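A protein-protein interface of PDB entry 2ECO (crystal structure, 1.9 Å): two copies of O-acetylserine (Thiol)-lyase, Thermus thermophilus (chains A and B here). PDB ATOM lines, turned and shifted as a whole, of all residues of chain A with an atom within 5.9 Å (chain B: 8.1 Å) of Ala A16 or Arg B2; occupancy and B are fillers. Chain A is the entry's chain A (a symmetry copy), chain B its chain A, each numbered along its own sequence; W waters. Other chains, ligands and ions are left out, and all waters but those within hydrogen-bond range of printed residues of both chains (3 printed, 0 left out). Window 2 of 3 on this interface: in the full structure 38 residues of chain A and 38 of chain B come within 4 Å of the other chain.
O of Ser B83 lies within hydrogen-bond range of NZ of Lys A17 (2.7 Å).
The backbone carbonyl oxygen of Ala B82 sits at hydrogen-bond distance from the side-chain amino group of Lys A17 (3.3 Å).
The backbone NH (N) of Arg A14 is in hydrogen-bond range of the backbone carbonyl oxygen (O) of Met B1 (2.8 Å).
OG of Ser B83 lies within hydrogen-bond range of OE1 of Glu B4, at 2.6 Å.
N of Val A18 lies within hydrogen-bond range of OE1 of Glu A256, 2.9 Å away.
The side-chain carboxylate (OE2) of Glu A256 is in hydrogen-bond range of the backbone NH (N) of Ala A16, at 3.0 Å.
The backbone NH (N) of Lys A17 sits at hydrogen-bond distance from the side-chain carboxylate (OE1) of Glu A256 (2.7 Å).
Among the printed residues, pairs that only touch across the chains: Val A13 with Met B1 (3.2 Å), Ala A16 with Arg B2 (3.3 Å), Lys A17 with Arg B2 (3.6 Å), Glu A256 with Ser B83 (3.6 Å), Glu A256 with Val B3 (3.7 Å), Val A13 with Arg B2 (3.9 Å) and Val A13 with Val B3 (3.99 Å).
Ala A16 touches one residue of chain B.
Of chain A, only Val A13, Ala A16 and Lys A17 come within 4 Å of Arg B2.
Of the printed residues of chain B, Glu A256 touches Val B3 and Ser B83.
Of the printed residues of chain A, Met B1 touches Val A13 (3.2 Å) and Arg A14 (2.8 Å).
Printed residues of chain B within 4 Å of Val A13: Met B1 (3.2 Å), Arg B2 (3.9 Å) and Val B3 (3.99 Å).
Printed residues of chain B within 4 Å of Arg A14: Met B1.
Of the printed residues of chain A, Val B3 touches Val A13 (3.99 Å) and Glu A256 (3.7 Å).
Of the 15 printed residues of chain B, 5 touch a printed residue of chain A.
Printed residues of chain B that touch a printed residue of chain A: Met B1, Arg B2, Val B3, Ala B82 and Ser B83.
Hydrophobic or aromatic side chains of chain B that line the printed part of chain A: Met B1 and Val B3.
Of the 8 printed residues of chain A, 5 touch a printed residue of chain B.
Hydrophobic or aromatic side chains of chain A within 4 Å of the printed part of chain B: Val A13 and Ala A16.
Among the printed residues, no Asp or Glu carboxylate lies within 4 Å of a Lys or Arg side-chain nitrogen of the other chain.
No position is printed for both chains.
Of the 10 pairs that touch across the chains among the printed residues, none has its exchanged pair printed and touching as well.
Water W1 lies within hydrogen-bond range of the backbone carbonyl oxygen (O) of Glu A256 (2.7 Å) and the backbone NH (N) of Val B3 (2.8 Å).
Water W2 lies within hydrogen-bond range of OG of Ser B83 (2.9 Å) and NZ of Lys A17 (3.4 Å).
Water W3 lies within hydrogen-bond range of the backbone carbonyl oxygen (O) of Arg A14 and the guanidinium group (NE) of Arg B2.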
ATOM      1  N   VAL A  13      25.532  -2.765   9.272  1.00  0.00           N
ATOM      2  CA  VAL A  13      25.510  -2.935   7.828  1.00  0.00           C
ATOM      3  C   VAL A  13      25.396  -4.408   7.451  1.00  0.00           C
ATOM      4  O   VAL A  13      25.858  -5.283   8.186  1.00  0.00           O
ATOM      5  CB  VAL A  13      26.786  -2.344   7.193  1.00  0.00           C
ATOM      6  CG1 VAL A  13      26.823  -0.835   7.420  1.00  0.00           C
ATOM      7  CG2 VAL A  13      28.021  -2.994   7.800  1.00  0.00           C
ATOM      8  N   ARG A  14      24.770  -4.680   6.308  1.00  0.00           N
ATOM      9  CA  ARG A  14      24.612  -6.054   5.840  1.00  0.00           C
ATOM     10  C   ARG A  14      25.635  -6.357   4.754  1.00  0.00           C
ATOM     11  O   ARG A  14      25.748  -5.618   3.774  1.00  0.00           O
ATOM     12  CB  ARG A  14      23.203  -6.282   5.282  1.00  0.00           C
ATOM     13  CG  ARG A  14      23.003  -7.695   4.738  1.00  0.00           C
ATOM     14  CD  ARG A  14      21.612  -7.908   4.152  1.00  0.00           C
ATOM     15  NE  ARG A  14      21.523  -9.215   3.504  1.00  0.00           N
ATOM     16  CZ  ARG A  14      20.471  -9.646   2.816  1.00  0.00           C
ATOM     17  NH1 ARG A  14      19.401  -8.876   2.679  1.00  0.00           N
ATOM     18  NH2 ARG A  14      20.492 -10.852   2.261  1.00  0.00           N
ATOM     19  N   LEU A  15      26.384  -7.441   4.928  1.00  0.00           N
ATOM     20  CA  LEU A  15      27.394  -7.818   3.948  1.00  0.00           C
ATOM     21  C   LEU A  15      26.686  -8.235   2.663  1.00  0.00           C
ATOM     22  O   LEU A  15      25.600  -8.818   2.710  1.00  0.00           O
ATOM     23  CB  LEU A  15      28.250  -8.966   4.481  1.00  0.00           C
ATOM     24  CG  LEU A  15      28.968  -8.669   5.808  1.00  0.00           C
ATOM     25  CD1 LEU A  15      29.887  -9.827   6.157  1.00  0.00           C
ATOM     26  CD2 LEU A  15      29.771  -7.374   5.685  1.00  0.00           C
ATOM     27  N   ALA A  16      27.307  -7.950   1.524  1.00  0.00           N
ATOM     28  CA  ALA A  16      26.702  -8.268   0.238  1.00  0.00           C
ATOM     29  C   ALA A  16      27.630  -8.939  -0.771  1.00  0.00           C
ATOM     30  O   ALA A  16      27.159  -9.506  -1.762  1.00  0.00           O
ATOM     31  CB  ALA A  16      26.121  -6.995  -0.368  1.00  0.00           C
ATOM     32  N   LYS A  17      28.937  -8.883  -0.535  1.00  0.00           N
ATOM     33  CA  LYS A  17      29.888  -9.475  -1.470  1.00  0.00           C
ATOM     34  C   LYS A  17      30.640 -10.694  -0.955  1.00  0.00           C
ATOM     35  O   LYS A  17      30.852 -11.642  -1.704  1.00  0.00           O
ATOM     36  CB  LYS A  17      30.903  -8.425  -1.943  1.00  0.00           C
ATOM     37  CG  LYS A  17      30.332  -7.347  -2.860  1.00  0.00           C
ATOM     38  CD  LYS A  17      29.440  -6.386  -2.092  1.00  0.00           C
ATOM     39  CE  LYS A  17      29.137  -5.146  -2.906  1.00  0.00           C
ATOM     40  NZ  LYS A  17      30.376  -4.410  -3.283  1.00  0.00           N
ATOM     41  N   VAL A  18      31.059 -10.671   0.310  1.00  0.00           N
ATOM     42  CA  VAL A  18      31.792 -11.807   0.865  1.00  0.00           C
ATOM     43  C   VAL A  18      30.865 -12.957   1.254  1.00  0.00           C
ATOM     44  O   VAL A  18      31.326 -14.049   1.581  1.00  0.00           O
ATOM     45  CB  VAL A  18      32.639 -11.405   2.101  1.00  0.00           C
ATOM     46  CG1 VAL A  18      33.632 -10.311   1.712  1.00  0.00           C
ATOM     47  CG2 VAL A  18      31.735 -10.952   3.245  1.00  0.00           C
ATOM     48  N   VAL A  19      29.560 -12.711   1.219  1.00  0.00           N
ATOM     49  CA  VAL A  19      28.593 -13.748   1.556  1.00  0.00           C
ATOM     50  C   VAL A  19      28.137 -14.457   0.291  1.00  0.00           C
ATOM     51  O   VAL A  19      28.351 -13.967  -0.819  1.00  0.00           O
ATOM     52  CB  VAL A  19      27.351 -13.172   2.263  1.00  0.00           C
ATOM     53  CG1 VAL A  19      27.745 -12.597   3.619  1.00  0.00           C
ATOM     54  CG2 VAL A  19      26.703 -12.103   1.396  1.00  0.00           C
ATOM     55  N   GLU A 256      33.444  -4.660   0.407  1.00  0.00           N
ATOM     56  CA  GLU A 256      32.302  -4.085   1.123  1.00  0.00           C
ATOM     57  C   GLU A 256      32.546  -2.628   1.510  1.00  0.00           C
ATOM     58  O   GLU A 256      31.628  -1.933   1.937  1.00  0.00           O
ATOM     59  CB  GLU A 256      32.017  -4.872   2.408  1.00  0.00           C
ATOM     60  CG  GLU A 256      31.967  -6.389   2.251  1.00  0.00           C
ATOM     61  CD  GLU A 256      30.634  -6.909   1.735  1.00  0.00           C
ATOM     62  OE1 GLU A 256      30.540  -8.132   1.512  1.00  0.00           O
ATOM     63  OE2 GLU A 256      29.683  -6.115   1.560  1.00  0.00           O
ATOM     64  N   MET B   1      21.449  -2.526   4.902  1.00  0.00           N
ATOM     65  CA  MET B   1      22.106  -1.214   4.655  1.00  0.00           C
ATOM     66  C   MET B   1      23.587  -1.429   4.361  1.00  0.00           C
ATOM     67  O   MET B   1      24.213  -2.324   4.920  1.00  0.00           O
ATOM     68  CB  MET B   1      21.944  -0.312   5.881  1.00  0.00           C
ATOM     69  CG  MET B   1      22.552   1.070   5.727  1.00  0.00           C
ATOM     70  SD  MET B   1      22.343   2.097   7.200  1.00  0.00           S
ATOM     71  CE  MET B   1      23.849   1.720   8.077  1.00  0.00           C
ATOM     72  N   ARG B   2      24.141  -0.617   3.469  1.00  0.00           N
ATOM     73  CA  ARG B   2      25.554  -0.735   3.129  1.00  0.00           C
ATOM     74  C   ARG B   2      26.331   0.415   3.762  1.00  0.00           C
ATOM     75  O   ARG B   2      25.734   1.342   4.299  1.00  0.00           O
ATOM     76  CB  ARG B   2      25.720  -0.780   1.610  1.00  0.00           C
ATOM     77  CG  ARG B   2      25.012  -1.999   1.020  1.00  0.00           C
ATOM     78  CD  ARG B   2      25.404  -2.284  -0.404  1.00  0.00           C
ATOM     79  NE  ARG B   2      24.729  -3.481  -0.910  1.00  0.00           N
ATOM     80  CZ  ARG B   2      24.986  -4.039  -2.088  1.00  0.00           C
ATOM     81  NH1 ARG B   2      25.906  -3.507  -2.880  1.00  0.00           N
ATOM     82  NH2 ARG B   2      24.324  -5.127  -2.473  1.00  0.00           N
ATOM     83  N   VAL B   3      27.657   0.352   3.703  1.00  0.00           N
ATOM     84  CA  VAL B   3      28.483   1.373   4.335  1.00  0.00           C
ATOM     85  C   VAL B   3      28.115   2.810   3.974  1.00  0.00           C
ATOM     86  O   VAL B   3      28.171   3.696   4.830  1.00  0.00           O
ATOM     87  CB  VAL B   3      29.990   1.136   4.050  1.00  0.00           C
ATOM     88  CG1 VAL B   3      30.312   1.456   2.602  1.00  0.00           C
ATOM     89  CG2 VAL B   3      30.835   1.979   4.997  1.00  0.00           C
ATOM     90  N   GLU B   4      27.736   3.052   2.720  1.00  0.00           N
ATOM     91  CA  GLU B   4      27.365   4.404   2.308  1.00  0.00           C
ATOM     92  C   GLU B   4      26.187   4.901   3.136  1.00  0.00           C
ATOM     93  O   GLU B   4      26.022   6.104   3.338  1.00  0.00           O
ATOM     94  CB  GLU B   4      27.010   4.448   0.815  1.00  0.00           C
ATOM     95  CG  GLU B   4      26.023   3.370   0.380  1.00  0.00           C
ATOM     96  CD  GLU B   4      26.714   2.168  -0.228  1.00  0.00           C
ATOM     97  OE1 GLU B   4      27.781   1.767   0.286  1.00  0.00           O
ATOM     98  OE2 GLU B   4      26.186   1.617  -1.219  1.00  0.00           O
ATOM     99  N   GLY B   5      25.367   3.973   3.622  1.00  0.00           N
ATOM    100  CA  GLY B   5      24.229   4.361   4.438  1.00  0.00           C
ATOM    101  C   GLY B   5      24.626   4.717   5.863  1.00  0.00           C
ATOM    102  O   GLY B   5      23.827   5.268   6.621  1.00  0.00           O
ATOM    103  N   ALA B   6      25.864   4.404   6.233  1.00  0.00           N
ATOM    104  CA  ALA B   6      26.360   4.691   7.576  1.00  0.00           C
ATOM    105  C   ALA B   6      27.003   6.072   7.665  1.00  0.00           C
ATOM    106  O   ALA B   6      27.532   6.459   8.712  1.00  0.00           O
ATOM    107  CB  ALA B   6      27.369   3.629   7.996  1.00  0.00           C
ATOM    108  N   ILE B   7      26.966   6.811   6.561  1.00  0.00           N
ATOM    109  CA  ILE B   7      27.543   8.150   6.511  1.00  0.00           C
ATOM    110  C   ILE B   7      26.573   9.193   7.065  1.00  0.00           C
ATOM    111  O   ILE B   7      25.368   9.116   6.826  1.00  0.00           O
ATOM    112  CB  ILE B   7      27.886   8.551   5.052  1.00  0.00           C
ATOM    113  CG1 ILE B   7      28.911   7.577   4.462  1.00  0.00           C
ATOM    114  CG2 ILE B   7      28.408   9.982   5.008  1.00  0.00           C
ATOM    115  CD1 ILE B   7      29.185   7.813   2.980  1.00  0.00           C
ATOM    116  N   PRO B  35      32.251   6.447   8.459  1.00  0.00           N
ATOM    117  CA  PRO B  35      32.914   5.192   8.090  1.00  0.00           C
ATOM    118  C   PRO B  35      34.231   5.358   7.340  1.00  0.00           C
ATOM    119  O   PRO B  35      35.106   4.496   7.419  1.00  0.00           O
ATOM    120  CB  PRO B  35      31.848   4.463   7.270  1.00  0.00           C
ATOM    121  CG  PRO B  35      31.046   5.585   6.677  1.00  0.00           C
ATOM    122  CD  PRO B  35      30.918   6.542   7.837  1.00  0.00           C
ATOM    123  N   PRO B  59      25.933   1.324 -10.600  1.00  0.00           N
ATOM    124  CA  PRO B  59      26.701   0.515  -9.648  1.00  0.00           C
ATOM    125  C   PRO B  59      26.864  -0.960 -10.018  1.00  0.00           C
ATOM    126  O   PRO B  59      25.980  -1.559 -10.636  1.00  0.00           O
ATOM    127  CB  PRO B  59      25.937   0.715  -8.341  1.00  0.00           C
ATOM    128  CG  PRO B  59      24.523   0.839  -8.810  1.00  0.00           C
ATOM    129  CD  PRO B  59      24.660   1.764 -10.001  1.00  0.00           C
ATOM    130  N   GLY B  60      28.006  -1.529  -9.637  1.00  0.00           N
ATOM    131  CA  GLY B  60      28.289  -2.927  -9.920  1.00  0.00           C
ATOM    132  C   GLY B  60      28.754  -3.156 -11.346  1.00  0.00           C
ATOM    133  O   GLY B  60      28.900  -4.296 -11.794  1.00  0.00           O
ATOM    134  N   ILE B  80      33.559   4.117  -1.158  1.00  0.00           N
ATOM    135  CA  ILE B  80      32.344   4.020  -1.963  1.00  0.00           C
ATOM    136  C   ILE B  80      32.549   3.146  -3.203  1.00  0.00           C
ATOM    137  O   ILE B  80      31.679   2.352  -3.560  1.00  0.00           O
ATOM    138  CB  ILE B  80      31.858   5.423  -2.414  1.00  0.00           C
ATOM    139  CG1 ILE B  80      31.587   6.310  -1.194  1.00  0.00           C
ATOM    140  CG2 ILE B  80      30.590   5.291  -3.253  1.00  0.00           C
ATOM    141  CD1 ILE B  80      30.485   5.806  -0.284  1.00  0.00           C
ATOM    142  N   ALA B  82      34.588   0.717  -3.514  1.00  0.00           N
ATOM    143  CA  ALA B  82      34.696  -0.668  -3.074  1.00  0.00           C
ATOM    144  C   ALA B  82      33.296  -1.221  -2.836  1.00  0.00           C
ATOM    145  O   ALA B  82      32.965  -2.321  -3.271  1.00  0.00           O
ATOM    146  CB  ALA B  82      35.523  -0.755  -1.785  1.00  0.00           C
ATOM    147  N   SER B  83      32.467  -0.440  -2.157  1.00  0.00           N
ATOM    148  CA  SER B  83      31.110  -0.868  -1.856  1.00  0.00           C
ATOM    149  C   SER B  83      30.192  -0.976  -3.065  1.00  0.00           C
ATOM    150  O   SER B  83      29.388  -1.899  -3.151  1.00  0.00           O
ATOM    151  CB  SER B  83      30.464   0.080  -0.847  1.00  0.00           C
ATOM    152  OG  SER B  83      29.124  -0.312  -0.595  1.00  0.00           O
ATOM    153  N   ARG B  84      30.304  -0.039  -3.999  1.00  0.00           N
ATOM    154  CA  ARG B  84      29.419  -0.058  -5.152  1.00  0.00           C
ATOM    155  C   ARG B  84      29.962  -0.677  -6.430  1.00  0.00           C
ATOM    156  O   ARG B  84      29.324  -0.601  -7.478  1.00  0.00           O
ATOM    157  CB  ARG B  84      28.893   1.350  -5.404  1.00  0.00           C
ATOM    158  CG  ARG B  84      28.127   1.885  -4.201  1.00  0.00           C
ATOM    159  CD  ARG B  84      27.527   3.244  -4.467  1.00  0.00           C
ATOM    160  NE  ARG B  84      26.313   3.186  -5.281  1.00  0.00           N
ATOM    161  CZ  ARG B  84      25.154   2.681  -4.873  1.00  0.00           C
ATOM    162  NH1 ARG B  84      25.038   2.172  -3.651  1.00  0.00           N
ATOM    163  NH2 ARG B  84      24.096   2.715  -5.675  1.00  0.00           N
ATOM    164  N   GLY B  85      31.136  -1.291  -6.338  1.00  0.00           N
ATOM    165  CA  GLY B  85      31.715  -1.968  -7.485  1.00  0.00           C
ATOM    166  C   GLY B  85      32.302  -1.176  -8.638  1.00  0.00           C
ATOM    167  O   GLY B  85      32.093  -1.526  -9.802  1.00  0.00           O
HETATM  168  O   HOH W   1      29.020  -1.884   2.585  1.00  0.00           O
HETATM  169  O   HOH W   2      28.914  -3.217  -0.449  1.00  0.00           O
HETATM  170  O   HOH W   3      23.584  -5.334   1.794  1.00  0.00           O
